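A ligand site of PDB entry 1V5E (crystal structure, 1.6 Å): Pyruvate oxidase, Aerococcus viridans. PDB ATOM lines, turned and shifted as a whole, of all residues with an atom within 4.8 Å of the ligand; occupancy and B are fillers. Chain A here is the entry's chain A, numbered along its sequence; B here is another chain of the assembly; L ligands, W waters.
Water W2 bridges the side-chain carboxylate (OD2) of Asp 301 (2.7 Å) and an oxygen (O6) of the ligand (2.8 Å).
Water W7 lies within hydrogen-bond range of the backbone carbonyl oxygen (O) of Thr 236, an oxygen (O7) of the ligand and the backbone NH (N) of Thr 255.
Water W6 lies within hydrogen-bond range of ND2 of Asn 279 (2.9 Å) and O2 of the ligand (2.9 Å).
Water W4 bridges OE1 of Gln 392 and O of Gly 238.
The backbone NH (N) of Gly 317 is in hydrogen-bond range of the backbone carbonyl oxygen (O) of Asp 299, at 3.0 Å.
The backbone NH (N) of Ile 214 is in hydrogen-bond range of the backbone carbonyl oxygen (O) of Gly 277, at 3.3 Å.
OD1 of Asn 279 sits close to SD of Met 304, at 3.4 Å.
OD1 of Asp 299 is in hydrogen-bond range of N of Asp 301, at 2.8 Å.
The backbone carbonyl oxygen of Gly 213 sits at hydrogen-bond distance from the side-chain amide nitrogen of Asn 240 (3.1 Å).
The backbone carbonyl oxygen of Ile 298 sits at hydrogen-bond distance from the backbone NH of Gly 277, 2.9 Å away.
The backbone carbonyl oxygen (O) of Gly 277 sits at hydrogen-bond distance from the backbone NH (N) of Gly 215 (3.0 Å).
The side-chain hydroxyl of Ser 278 lies within hydrogen-bond range of the backbone NH of Phe 280.
The side-chain carboxylate of Asp 318 is in hydrogen-bond range of a nitrogen (N3) of the ligand (3.0 Å).
O5 of the ligand is in hydrogen-bond range of OD2 of Asp 299 (2.7 Å).
The side-chain amino group (NZ) of Lys 239 is in salt-bridge range of an oxygen (O1) of the ligand, at 2.8 Å.
O9 of the ligand sits at hydrogen-bond distance from O of Pro 410, 2.7 Å away.
The backbone NH (N) of Asn 279 lies within hydrogen-bond range of an oxygen (O13) of the ligand, at 2.9 Å.
The backbone NH of Ile 300 lies within hydrogen-bond range of a nitrogen (N5) of the ligand (3.5 Å).
The backbone carbonyl oxygen of Thr 255 is in hydrogen-bond range of a nitrogen (N7) of the ligand, at 2.9 Å.
N of Ile 214 lies within hydrogen-bond range of O14 of the ligand (2.7 Å).
N of Ala 319 sits at hydrogen-bond distance from N4 of the ligand (2.9 Å).
The backbone NH (N) of Gly 238 sits at hydrogen-bond distance from an oxygen (O7) of the ligand (3.2 Å).
N of Arg 257 sits at hydrogen-bond distance from O8 of the ligand (3.3 Å).
The side-chain hydroxyl (OG) of Ser 278 sits at hydrogen-bond distance from an oxygen (O13) of the ligand (2.7 Å).
The backbone carbonyl oxygen of Val 258 sits close to a nitrogen (N7) of the ligand (3.3 Å).
OG1 of Thr 237 is in hydrogen-bond range of O14 of the ligand (2.6 Å).
N of Val 258 sits at hydrogen-bond distance from O8 of the ligand (2.5 Å).
The side-chain sulfur (SD) of Met 304 lies close to an oxygen (O5) of the ligand (3.7 Å).
The backbone carbonyl oxygen (O) of Gly 277 sits close to an oxygen (O4) of the ligand (3.1 Å).
Residues that only touch the ligand: Gly 213, Gly 215, Tyr 256, Phe 280, Pro 281, Phe 282, Asp 301, Gly 317, Val 387, Ser 409, Ala 413 and Phe 114 of chain B.
The nearest printed residue that does not touch the ligand is Ser 254 (4.01 Å).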
ATOM      1  N   GLY A 213     -26.372   5.505 -11.399  1.00  0.00           N
ATOM      2  CA  GLY A 213     -25.195   6.130 -11.984  1.00  0.00           C
ATOM      3  C   GLY A 213     -25.424   6.363 -13.470  1.00  0.00           C
ATOM      4  O   GLY A 213     -26.519   6.087 -13.961  1.00  0.00           O
ATOM      5  N   ILE A 214     -24.422   6.842 -14.196  1.00  0.00           N
ATOM      6  CA  ILE A 214     -24.608   7.144 -15.607  1.00  0.00           C
ATOM      7  C   ILE A 214     -24.984   5.961 -16.501  1.00  0.00           C
ATOM      8  O   ILE A 214     -25.274   6.143 -17.685  1.00  0.00           O
ATOM      9  CB  ILE A 214     -23.385   7.856 -16.229  1.00  0.00           C
ATOM     10  CG1 ILE A 214     -22.156   6.950 -16.210  1.00  0.00           C
ATOM     11  CG2 ILE A 214     -23.121   9.155 -15.470  1.00  0.00           C
ATOM     12  CD1 ILE A 214     -21.065   7.407 -17.173  1.00  0.00           C
ATOM     13  N   GLY A 215     -25.000   4.756 -15.930  1.00  0.00           N
ATOM     14  CA  GLY A 215     -25.405   3.609 -16.716  1.00  0.00           C
ATOM     15  C   GLY A 215     -26.889   3.729 -17.006  1.00  0.00           C
ATOM     16  O   GLY A 215     -27.427   3.062 -17.895  1.00  0.00           O
ATOM     17  N   THR A 236     -28.519   9.730  -6.787  1.00  0.00           N
ATOM     18  CA  THR A 236     -27.782   9.747  -8.040  1.00  0.00           C
ATOM     19  C   THR A 236     -26.308   9.972  -7.738  1.00  0.00           C
ATOM     20  O   THR A 236     -25.915  10.127  -6.587  1.00  0.00           O
ATOM     21  CB  THR A 236     -28.300  10.862  -8.991  1.00  0.00           C
ATOM     22  OG1 THR A 236     -27.605  10.803 -10.237  1.00  0.00           O
ATOM     23  CG2 THR A 236     -28.092  12.234  -8.365  1.00  0.00           C
ATOM     24  N   THR A 237     -25.477   9.964  -8.774  1.00  0.00           N
ATOM     25  CA  THR A 237     -24.045  10.192  -8.605  1.00  0.00           C
ATOM     26  C   THR A 237     -23.708  11.588  -9.111  1.00  0.00           C
ATOM     27  O   THR A 237     -24.505  12.222  -9.789  1.00  0.00           O
ATOM     28  CB  THR A 237     -23.231   9.176  -9.411  1.00  0.00           C
ATOM     29  OG1 THR A 237     -23.571   9.304 -10.795  1.00  0.00           O
ATOM     30  CG2 THR A 237     -23.513   7.766  -8.934  1.00  0.00           C
ATOM     31  N   GLY A 238     -22.510  12.061  -8.771  1.00  0.00           N
ATOM     32  CA  GLY A 238     -22.084  13.372  -9.218  1.00  0.00           C
ATOM     33  C   GLY A 238     -22.012  13.533 -10.728  1.00  0.00           C
ATOM     34  O   GLY A 238     -21.954  14.650 -11.221  1.00  0.00           O
ATOM     35  N   LYS A 239     -22.021  12.423 -11.458  1.00  0.00           N
ATOM     36  CA  LYS A 239     -21.967  12.465 -12.915  1.00  0.00           C
ATOM     37  C   LYS A 239     -23.323  12.329 -13.587  1.00  0.00           C
ATOM     38  O   LYS A 239     -23.476  12.650 -14.763  1.00  0.00           O
ATOM     39  CB  LYS A 239     -21.098  11.318 -13.467  1.00  0.00           C
ATOM     40  CG  LYS A 239     -19.610  11.420 -13.188  1.00  0.00           C
ATOM     41  CD  LYS A 239     -18.862  10.193 -13.711  1.00  0.00           C
ATOM     42  CE  LYS A 239     -18.948  10.051 -15.230  1.00  0.00           C
ATOM     43  NZ  LYS A 239     -18.141   8.877 -15.716  1.00  0.00           N
ATOM     44  N   ASN A 240     -24.322  11.884 -12.828  1.00  0.00           N
ATOM     45  CA  ASN A 240     -25.641  11.575 -13.375  1.00  0.00           C
ATOM     46  C   ASN A 240     -26.872  12.440 -13.035  1.00  0.00           C
ATOM     47  O   ASN A 240     -28.002  11.974 -13.183  1.00  0.00           O
ATOM     48  CB  ASN A 240     -25.934  10.115 -13.005  1.00  0.00           C
ATOM     49  CG  ASN A 240     -26.999   9.488 -13.875  1.00  0.00           C
ATOM     50  OD1 ASN A 240     -26.962   9.596 -15.097  1.00  0.00           O
ATOM     51  ND2 ASN A 240     -27.938   8.796 -13.246  1.00  0.00           N
ATOM     52  N   SER A 254     -27.001  13.331  -4.380  1.00  0.00           N
ATOM     53  CA  SER A 254     -25.890  12.388  -4.360  1.00  0.00           C
ATOM     54  C   SER A 254     -25.292  12.323  -2.963  1.00  0.00           C
ATOM     55  O   SER A 254     -25.509  13.227  -2.142  1.00  0.00           O
ATOM     56  CB  SER A 254     -24.827  12.813  -5.383  1.00  0.00           C
ATOM     57  OG  SER A 254     -24.515  14.191  -5.258  1.00  0.00           O
ATOM     58  N   THR A 255     -24.527  11.266  -2.672  1.00  0.00           N
ATOM     59  CA  THR A 255     -23.923  11.139  -1.348  1.00  0.00           C
ATOM     60  C   THR A 255     -22.509  11.703  -1.292  1.00  0.00           C
ATOM     61  O   THR A 255     -21.906  12.011  -2.318  1.00  0.00           O
ATOM     62  CB  THR A 255     -23.907   9.667  -0.853  1.00  0.00           C
ATOM     63  OG1 THR A 255     -22.914   8.913  -1.554  1.00  0.00           O
ATOM     64  CG2 THR A 255     -25.272   9.029  -1.045  1.00  0.00           C
ATOM     65  N   TYR A 256     -22.003  11.814  -0.064  1.00  0.00           N
ATOM     66  CA  TYR A 256     -20.687  12.367   0.266  1.00  0.00           C
ATOM     67  C   TYR A 256     -20.638  13.878   0.015  1.00  0.00           C
ATOM     68  O   TYR A 256     -21.693  14.521  -0.087  1.00  0.00           O
ATOM     69  CB  TYR A 256     -19.547  11.637  -0.491  1.00  0.00           C
ATOM     70  CG  TYR A 256     -18.199  11.865   0.173  1.00  0.00           C
ATOM     71  CD1 TYR A 256     -18.043  11.710   1.552  1.00  0.00           C
ATOM     72  CD2 TYR A 256     -17.097  12.281  -0.563  1.00  0.00           C
ATOM     73  CE1 TYR A 256     -16.833  11.986   2.184  1.00  0.00           C
ATOM     74  CE2 TYR A 256     -15.873  12.561   0.052  1.00  0.00           C
ATOM     75  CZ  TYR A 256     -15.754  12.415   1.433  1.00  0.00           C
ATOM     76  OH  TYR A 256     -14.556  12.708   2.053  1.00  0.00           O
ATOM     77  N   ARG A 257     -19.437  14.443  -0.073  1.00  0.00           N
ATOM     78  CA  ARG A 257     -19.212  15.887  -0.244  1.00  0.00           C
ATOM     79  C   ARG A 257     -19.962  16.617  -1.359  1.00  0.00           C
ATOM     80  O   ARG A 257     -20.677  17.582  -1.087  1.00  0.00           O
ATOM     81  CB  ARG A 257     -17.717  16.146  -0.367  1.00  0.00           C
ATOM     82  CG  ARG A 257     -16.931  15.716   0.853  1.00  0.00           C
ATOM     83  CD  ARG A 257     -15.433  15.912   0.676  1.00  0.00           C
ATOM     84  NE  ARG A 257     -15.067  17.305   0.445  1.00  0.00           N
ATOM     85  CZ  ARG A 257     -13.824  17.722   0.257  1.00  0.00           C
ATOM     86  NH1 ARG A 257     -12.823  16.848   0.274  1.00  0.00           N
ATOM     87  NH2 ARG A 257     -13.580  19.004   0.053  1.00  0.00           N
ATOM     88  N   VAL A 258     -19.758  16.209  -2.605  1.00  0.00           N
ATOM     89  CA  VAL A 258     -20.467  16.837  -3.705  1.00  0.00           C
ATOM     90  C   VAL A 258     -21.781  16.083  -3.776  1.00  0.00           C
ATOM     91  O   VAL A 258     -22.001  15.215  -4.629  1.00  0.00           O
ATOM     92  CB  VAL A 258     -19.705  16.712  -5.040  1.00  0.00           C
ATOM     93  CG1 VAL A 258     -20.550  17.262  -6.187  1.00  0.00           C
ATOM     94  CG2 VAL A 258     -18.401  17.474  -4.941  1.00  0.00           C
ATOM     95  N   GLY A 259     -22.652  16.411  -2.828  1.00  0.00           N
ATOM     96  CA  GLY A 259     -23.944  15.764  -2.745  1.00  0.00           C
ATOM     97  C   GLY A 259     -24.928  16.649  -1.995  1.00  0.00           C
ATOM     98  O   GLY A 259     -24.660  17.836  -1.786  1.00  0.00           O
ATOM     99  N   GLY A 277     -26.028   0.809 -12.707  1.00  0.00           N
ATOM    100  CA  GLY A 277     -25.057   1.483 -13.566  1.00  0.00           C
ATOM    101  C   GLY A 277     -24.185   2.514 -12.889  1.00  0.00           C
ATOM    102  O   GLY A 277     -24.134   3.663 -13.310  1.00  0.00           O
ATOM    103  N   SER A 278     -23.478   2.095 -11.842  1.00  0.00           N
ATOM    104  CA  SER A 278     -22.595   2.984 -11.106  1.00  0.00           C
ATOM    105  C   SER A 278     -21.300   2.303 -10.661  1.00  0.00           C
ATOM    106  O   SER A 278     -21.249   1.084 -10.506  1.00  0.00           O
ATOM    107  CB  SER A 278     -23.310   3.530  -9.864  1.00  0.00           C
ATOM    108  OG  SER A 278     -22.436   4.355  -9.093  1.00  0.00           O
ATOM    109  N   ASN A 279     -20.255   3.110 -10.497  1.00  0.00           N
ATOM    110  CA  ASN A 279     -18.985   2.623  -9.997  1.00  0.00           C
ATOM    111  C   ASN A 279     -18.490   3.679  -9.019  1.00  0.00           C
ATOM    112  O   ASN A 279     -17.310   4.020  -8.988  1.00  0.00           O
ATOM    113  CB  ASN A 279     -17.978   2.385 -11.125  1.00  0.00           C
ATOM    114  CG  ASN A 279     -16.723   1.662 -10.639  1.00  0.00           C
ATOM    115  OD1 ASN A 279     -16.807   0.791  -9.771  1.00  0.00           O
ATOM    116  ND2 ASN A 279     -15.576   2.003 -11.203  1.00  0.00           N
ATOM    117  N   PHE A 280     -19.435   4.178  -8.215  1.00  0.00           N
ATOM    118  CA  PHE A 280     -19.203   5.203  -7.188  1.00  0.00           C
ATOM    119  C   PHE A 280     -17.880   4.919  -6.480  1.00  0.00           C
ATOM    120  O   PHE A 280     -17.762   3.952  -5.723  1.00  0.00           O
ATOM    121  CB  PHE A 280     -20.376   5.172  -6.205  1.00  0.00           C
ATOM    122  CG  PHE A 280     -20.362   6.273  -5.185  1.00  0.00           C
ATOM    123  CD1 PHE A 280     -20.338   7.613  -5.583  1.00  0.00           C
ATOM    124  CD2 PHE A 280     -20.386   5.985  -3.824  1.00  0.00           C
ATOM    125  CE1 PHE A 280     -20.353   8.629  -4.636  1.00  0.00           C
ATOM    126  CE2 PHE A 280     -20.401   7.000  -2.877  1.00  0.00           C
ATOM    127  CZ  PHE A 280     -20.383   8.328  -3.277  1.00  0.00           C
ATOM    128  N   PRO A 281     -16.873   5.774  -6.695  1.00  0.00           N
ATOM    129  CA  PRO A 281     -15.542   5.615  -6.094  1.00  0.00           C
ATOM    130  C   PRO A 281     -15.373   5.805  -4.583  1.00  0.00           C
ATOM    131  O   PRO A 281     -14.358   5.385  -4.018  1.00  0.00           O
ATOM    132  CB  PRO A 281     -14.689   6.590  -6.886  1.00  0.00           C
ATOM    133  CG  PRO A 281     -15.644   7.724  -7.127  1.00  0.00           C
ATOM    134  CD  PRO A 281     -16.930   7.000  -7.519  1.00  0.00           C
ATOM    135  N   PHE A 282     -16.336   6.441  -3.932  1.00  0.00           N
ATOM    136  CA  PHE A 282     -16.223   6.662  -2.495  1.00  0.00           C
ATOM    137  C   PHE A 282     -16.823   5.528  -1.681  1.00  0.00           C
ATOM    138  O   PHE A 282     -16.667   5.493  -0.461  1.00  0.00           O
ATOM    139  CB  PHE A 282     -16.917   7.975  -2.120  1.00  0.00           C
ATOM    140  CG  PHE A 282     -16.304   9.193  -2.753  1.00  0.00           C
ATOM    141  CD1 PHE A 282     -15.161   9.771  -2.206  1.00  0.00           C
ATOM    142  CD2 PHE A 282     -16.861   9.753  -3.892  1.00  0.00           C
ATOM    143  CE1 PHE A 282     -14.586  10.895  -2.780  1.00  0.00           C
ATOM    144  CE2 PHE A 282     -16.291  10.874  -4.487  1.00  0.00           C
ATOM    145  CZ  PHE A 282     -15.150  11.452  -3.931  1.00  0.00           C
ATOM    146  N   ILE A 298     -26.702  -3.689 -11.132  1.00  0.00           N
ATOM    147  CA  ILE A 298     -26.957  -3.820 -12.558  1.00  0.00           C
ATOM    148  C   ILE A 298     -25.804  -3.145 -13.280  1.00  0.00           C
ATOM    149  O   ILE A 298     -25.489  -1.992 -12.999  1.00  0.00           O
ATOM    150  CB  ILE A 298     -28.245  -3.095 -13.000  1.00  0.00           C
ATOM    151  CG1 ILE A 298     -29.454  -3.672 -12.266  1.00  0.00           C
ATOM    152  CG2 ILE A 298     -28.405  -3.218 -14.506  1.00  0.00           C
ATOM    153  CD1 ILE A 298     -30.710  -2.821 -12.407  1.00  0.00           C
ATOM    154  N   ASP A 299     -25.169  -3.854 -14.209  1.00  0.00           N
ATOM    155  CA  ASP A 299     -24.054  -3.276 -14.955  1.00  0.00           C
ATOM    156  C   ASP A 299     -23.790  -4.075 -16.224  1.00  0.00           C
ATOM    157  O   ASP A 299     -24.095  -5.269 -16.278  1.00  0.00           O
ATOM    158  CB  ASP A 299     -22.792  -3.238 -14.084  1.00  0.00           C
ATOM    159  CG  ASP A 299     -21.833  -2.131 -14.484  1.00  0.00           C
ATOM    160  OD1 ASP A 299     -21.242  -2.187 -15.580  1.00  0.00           O
ATOM    161  OD2 ASP A 299     -21.671  -1.179 -13.683  1.00  0.00           O
ATOM    162  N   ILE A 300     -23.236  -3.425 -17.246  1.00  0.00           N
ATOM    163  CA  ILE A 300     -22.928  -4.114 -18.489  1.00  0.00           C
ATOM    164  C   ILE A 300     -21.507  -4.662 -18.460  1.00  0.00           C
ATOM    165  O   ILE A 300     -21.120  -5.460 -19.318  1.00  0.00           O
ATOM    166  CB  ILE A 300     -23.039  -3.171 -19.710  1.00  0.00           C
ATOM    167  CG1 ILE A 300     -22.185  -1.930 -19.491  1.00  0.00           C
ATOM    168  CG2 ILE A 300     -24.501  -2.843 -19.974  1.00  0.00           C
ATOM    169  CD1 ILE A 300     -22.095  -1.016 -20.695  1.00  0.00           C
ATOM    170  N   ASP A 301     -20.731  -4.231 -17.472  1.00  0.00           N
ATOM    171  CA  ASP A 301     -19.341  -4.648 -17.321  1.00  0.00           C
ATOM    172  C   ASP A 301     -19.188  -5.676 -16.197  1.00  0.00           C
ATOM    173  O   ASP A 301     -19.324  -5.354 -15.022  1.00  0.00           O
ATOM    174  CB  ASP A 301     -18.479  -3.413 -17.039  1.00  0.00           C
ATOM    175  CG  ASP A 301     -16.999  -3.722 -16.996  1.00  0.00           C
ATOM    176  OD1 ASP A 301     -16.613  -4.904 -17.099  1.00  0.00           O
ATOM    177  OD2 ASP A 301     -16.209  -2.756 -16.845  1.00  0.00           O
ATOM    178  N   MET A 304     -17.273  -5.000 -12.979  1.00  0.00           N
ATOM    179  CA  MET A 304     -17.873  -4.140 -11.963  1.00  0.00           C
ATOM    180  C   MET A 304     -18.808  -4.851 -10.984  1.00  0.00           C
ATOM    181  O   MET A 304     -19.105  -4.322  -9.910  1.00  0.00           O
ATOM    182  CB  MET A 304     -18.670  -3.022 -12.631  1.00  0.00           C
ATOM    183  CG  MET A 304     -17.857  -2.105 -13.527  1.00  0.00           C
ATOM    184  SD  MET A 304     -16.719  -1.095 -12.592  1.00  0.00           S
ATOM    185  CE  MET A 304     -15.195  -1.997 -12.800  1.00  0.00           C
ATOM    186  N   GLY A 317     -26.148  -6.684 -17.946  1.00  0.00           N
ATOM    187  CA  GLY A 317     -26.906  -6.254 -19.107  1.00  0.00           C
ATOM    188  C   GLY A 317     -27.207  -4.772 -19.052  1.00  0.00           C
ATOM    189  O   GLY A 317     -26.810  -4.075 -18.113  1.00  0.00           O
ATOM    190  N   ASP A 318     -27.932  -4.294 -20.060  1.00  0.00           N
ATOM    191  CA  ASP A 318     -28.291  -2.888 -20.146  1.00  0.00           C
ATOM    192  C   ASP A 318     -29.215  -2.454 -19.001  1.00  0.00           C
ATOM    193  O   ASP A 318     -30.180  -3.134 -18.665  1.00  0.00           O
ATOM    194  CB  ASP A 318     -28.953  -2.633 -21.498  1.00  0.00           C
ATOM    195  CG  ASP A 318     -29.296  -1.183 -21.702  1.00  0.00           C
ATOM    196  OD1 ASP A 318     -28.373  -0.378 -21.949  1.00  0.00           O
ATOM    197  OD2 ASP A 318     -30.486  -0.850 -21.593  1.00  0.00           O
ATOM    198  N   ALA A 319     -28.905  -1.293 -18.412  1.00  0.00           N
ATOM    199  CA  ALA A 319     -29.684  -0.751 -17.298  1.00  0.00           C
ATOM    200  C   ALA A 319     -31.117  -0.429 -17.711  1.00  0.00           C
ATOM    201  O   ALA A 319     -32.046  -0.588 -16.922  1.00  0.00           O
ATOM    202  CB  ALA A 319     -29.005   0.498 -16.741  1.00  0.00           C
ATOM    203  N   VAL A 387     -13.341  21.374 -11.798  1.00  0.00           N
ATOM    204  CA  VAL A 387     -13.276  20.563 -10.572  1.00  0.00           C
ATOM    205  C   VAL A 387     -13.185  21.176  -9.175  1.00  0.00           C
ATOM    206  O   VAL A 387     -13.031  20.449  -8.192  1.00  0.00           O
ATOM    207  CB  VAL A 387     -12.124  19.554 -10.711  1.00  0.00           C
ATOM    208  CG1 VAL A 387     -12.309  18.746 -11.995  1.00  0.00           C
ATOM    209  CG2 VAL A 387     -10.801  20.286 -10.731  1.00  0.00           C
ATOM    210  N   GLN A 392     -18.241  22.245  -8.470  1.00  0.00           N
ATOM    211  CA  GLN A 392     -18.854  20.937  -8.314  1.00  0.00           C
ATOM    212  C   GLN A 392     -20.170  21.073  -7.544  1.00  0.00           C
ATOM    213  O   GLN A 392     -21.093  20.274  -7.729  1.00  0.00           O
ATOM    214  CB  GLN A 392     -17.918  19.981  -7.596  1.00  0.00           C
ATOM    215  CG  GLN A 392     -16.812  19.426  -8.487  1.00  0.00           C
ATOM    216  CD  GLN A 392     -17.352  18.664  -9.670  1.00  0.00           C
ATOM    217  OE1 GLN A 392     -18.109  17.698  -9.524  1.00  0.00           O
ATOM    218  NE2 GLN A 392     -16.967  19.084 -10.876  1.00  0.00           N
ATOM    219  N   SER A 409     -14.425  16.482 -15.157  1.00  0.00           N
ATOM    220  CA  SER A 409     -13.337  15.491 -15.073  1.00  0.00           C
ATOM    221  C   SER A 409     -13.681  14.974 -13.686  1.00  0.00           C
ATOM    222  O   SER A 409     -13.151  15.453 -12.693  1.00  0.00           O
ATOM    223  CB  SER A 409     -11.960  16.168 -15.062  1.00  0.00           C
ATOM    224  OG  SER A 409     -10.940  15.203 -14.828  1.00  0.00           O
ATOM    225  N   PRO A 410     -14.571  13.973 -13.614  1.00  0.00           N
ATOM    226  CA  PRO A 410     -15.039  13.380 -12.363  1.00  0.00           C
ATOM    227  C   PRO A 410     -14.182  12.445 -11.529  1.00  0.00           C
ATOM    228  O   PRO A 410     -14.384  12.357 -10.326  1.00  0.00           O
ATOM    229  CB  PRO A 410     -16.323  12.687 -12.805  1.00  0.00           C
ATOM    230  CG  PRO A 410     -15.929  12.138 -14.145  1.00  0.00           C
ATOM    231  CD  PRO A 410     -15.149  13.284 -14.782  1.00  0.00           C
ATOM    232  N   LEU A 411     -13.239  11.761 -12.167  1.00  0.00           N
ATOM    233  CA  LEU A 411     -12.423  10.799 -11.436  1.00  0.00           C
ATOM    234  C   LEU A 411     -10.954  11.194 -11.333  1.00  0.00           C
ATOM    235  O   LEU A 411     -10.384  11.184 -10.240  1.00  0.00           O
ATOM    236  CB  LEU A 411     -12.565   9.426 -12.107  1.00  0.00           C
ATOM    237  CG  LEU A 411     -12.001   8.203 -11.367  1.00  0.00           C
ATOM    238  CD1 LEU A 411     -12.597   8.110  -9.970  1.00  0.00           C
ATOM    239  CD2 LEU A 411     -12.325   6.957 -12.169  1.00  0.00           C
ATOM    240  N   ALA A 413     -10.080  14.100 -12.128  1.00  0.00           N
ATOM    241  CA  ALA A 413     -10.321  15.448 -11.622  1.00  0.00           C
ATOM    242  C   ALA A 413      -9.254  16.476 -11.958  1.00  0.00           C
ATOM    243  O   ALA A 413      -8.762  17.181 -11.068  1.00  0.00           O
ATOM    244  CB  ALA A 413     -10.535  15.388 -10.111  1.00  0.00           C
ATOM    245  N   PHE B 114     -11.547   8.112  -5.332  1.00  0.00           N
ATOM    246  CA  PHE B 114     -11.493   9.378  -6.046  1.00  0.00           C
ATOM    247  C   PHE B 114     -10.072   9.907  -6.185  1.00  0.00           C
ATOM    248  O   PHE B 114      -9.323   9.972  -5.210  1.00  0.00           O
ATOM    249  CB  PHE B 114     -12.349  10.419  -5.320  1.00  0.00           C
ATOM    250  CG  PHE B 114     -12.209  11.792  -5.875  1.00  0.00           C
ATOM    251  CD1 PHE B 114     -12.654  12.088  -7.152  1.00  0.00           C
ATOM    252  CD2 PHE B 114     -11.568  12.792  -5.141  1.00  0.00           C
ATOM    253  CE1 PHE B 114     -12.469  13.350  -7.691  1.00  0.00           C
ATOM    254  CE2 PHE B 114     -11.377  14.056  -5.668  1.00  0.00           C
ATOM    255  CZ  PHE B 114     -11.828  14.340  -6.947  1.00  0.00           C
HETATM  256  P1  LIG L   1     -19.056   5.816 -13.497  1.00  0.00           P
HETATM  257  O1  LIG L   1     -18.651   6.312 -14.840  1.00  0.00           O
HETATM  258  O2  LIG L   1     -18.060   5.797 -12.404  1.00  0.00           O
HETATM  259  O3  LIG L   1     -19.586   4.325 -13.639  1.00  0.00           O
HETATM  260  C1  LIG L   1     -20.730   4.043 -14.441  1.00  0.00           C
HETATM  261  C2  LIG L   1     -21.024   2.571 -14.432  1.00  0.00           C
HETATM  262  O4  LIG L   1     -22.155   2.311 -15.313  1.00  0.00           O
HETATM  263  C3  LIG L   1     -19.881   1.672 -14.938  1.00  0.00           C
HETATM  264  O5  LIG L   1     -19.641   0.624 -14.001  1.00  0.00           O
HETATM  265  C4  LIG L   1     -20.370   1.184 -16.292  1.00  0.00           C
HETATM  266  O6  LIG L   1     -19.844  -0.068 -16.684  1.00  0.00           O
HETATM  267  C5  LIG L   1     -21.878   1.175 -16.109  1.00  0.00           C
HETATM  268  N1  LIG L   1     -22.667   1.299 -17.344  1.00  0.00           N
HETATM  269  C6  LIG L   1     -22.409   2.060 -18.453  1.00  0.00           C
HETATM  270  N2  LIG L   1     -23.316   1.956 -19.396  1.00  0.00           N
HETATM  271  C7  LIG L   1     -24.239   1.064 -18.864  1.00  0.00           C
HETATM  272  C8  LIG L   1     -25.461   0.526 -19.367  1.00  0.00           C
HETATM  273  N3  LIG L   1     -25.964   0.838 -20.565  1.00  0.00           N
HETATM  274  N4  LIG L   1     -26.142  -0.351 -18.571  1.00  0.00           N
HETATM  275  C9  LIG L   1     -25.629  -0.670 -17.360  1.00  0.00           C
HETATM  276  N5  LIG L   1     -24.493  -0.220 -16.789  1.00  0.00           N
HETATM  277  C10 LIG L   1     -23.849   0.645 -17.595  1.00  0.00           C
HETATM  278  N6  LIG L   1     -19.557  11.986  -6.902  1.00  0.00           N
HETATM  279  C11 LIG L   1     -20.450  11.720  -5.903  1.00  0.00           C
HETATM  280  O7  LIG L   1     -21.353  10.939  -6.062  1.00  0.00           O
HETATM  281  N7  LIG L   1     -20.309  12.385  -4.687  1.00  0.00           N
HETATM  282  C12 LIG L   1     -19.327  13.311  -4.430  1.00  0.00           C
HETATM  283  O8  LIG L   1     -19.256  13.866  -3.308  1.00  0.00           O
HETATM  284  C13 LIG L   1     -18.419  13.601  -5.476  1.00  0.00           C
HETATM  285  N8  LIG L   1     -17.435  14.557  -5.310  1.00  0.00           N
HETATM  286  C14 LIG L   1     -16.577  14.852  -6.337  1.00  0.00           C
HETATM  287  C15 LIG L   1     -15.611  15.833  -6.175  1.00  0.00           C
HETATM  288  C16 LIG L   1     -14.733  16.198  -7.203  1.00  0.00           C
HETATM  289  C17 LIG L   1     -13.711  17.284  -6.972  1.00  0.00           C
HETATM  290  C18 LIG L   1     -14.834  15.503  -8.452  1.00  0.00           C
HETATM  291  C19 LIG L   1     -13.928  15.842  -9.599  1.00  0.00           C
HETATM  292  C20 LIG L   1     -15.801  14.501  -8.626  1.00  0.00           C
HETATM  293  C21 LIG L   1     -16.688  14.154  -7.588  1.00  0.00           C
HETATM  294  N9  LIG L   1     -17.686  13.163  -7.738  1.00  0.00           N
HETATM  295  C22 LIG L   1     -18.570  12.902  -6.696  1.00  0.00           C
HETATM  296  C23 LIG L   1     -17.835  12.357  -8.993  1.00  0.00           C
HETATM  297  C24 LIG L   1     -17.262  10.979  -8.597  1.00  0.00           C
HETATM  298  O9  LIG L   1     -15.864  11.069  -8.412  1.00  0.00           O
HETATM  299  C25 LIG L   1     -17.541   9.895  -9.659  1.00  0.00           C
HETATM  300  O10 LIG L   1     -16.951  10.223 -10.913  1.00  0.00           O
HETATM  301  C26 LIG L   1     -19.009   9.640  -9.992  1.00  0.00           C
HETATM  302  O11 LIG L   1     -19.775   9.549  -8.780  1.00  0.00           O
HETATM  303  C27 LIG L   1     -19.109   8.340 -10.794  1.00  0.00           C
HETATM  304  O12 LIG L   1     -20.481   8.251 -11.169  1.00  0.00           O
HETATM  305  P2  LIG L   1     -21.202   6.997 -11.809  1.00  0.00           P
HETATM  306  O13 LIG L   1     -21.136   5.873 -10.855  1.00  0.00           O
HETATM  307  O14 LIG L   1     -22.516   7.469 -12.331  1.00  0.00           O
HETATM  308  O15 LIG L   1     -20.438   6.559 -13.127  1.00  0.00           O
HETATM  309  O   HOH W   1     -25.118   3.994 -21.788  1.00  0.00           O
HETATM  310  O   HOH W   2     -17.061  -0.172 -16.874  1.00  0.00           O
HETATM  311  O   HOH W   3     -17.894   5.132 -17.160  1.00  0.00           O
HETATM  312  O   HOH W   4     -19.011  15.171 -10.305  1.00  0.00           O
HETATM  313  O   HOH W   5     -19.701   3.863 -18.752  1.00  0.00           O
HETATM  314  O   HOH W   6     -15.872   4.059 -13.190  1.00  0.00           O
HETATM  315  O   HOH W   7     -23.651   9.587  -5.068  1.00  0.00           O
HETATM  316  O   HOH W   8     -15.897  14.775  -2.697  1.00  0.00           O
HETATM  317  O   HOH W   9     -16.101   7.731 -11.889  1.00  0.00           O
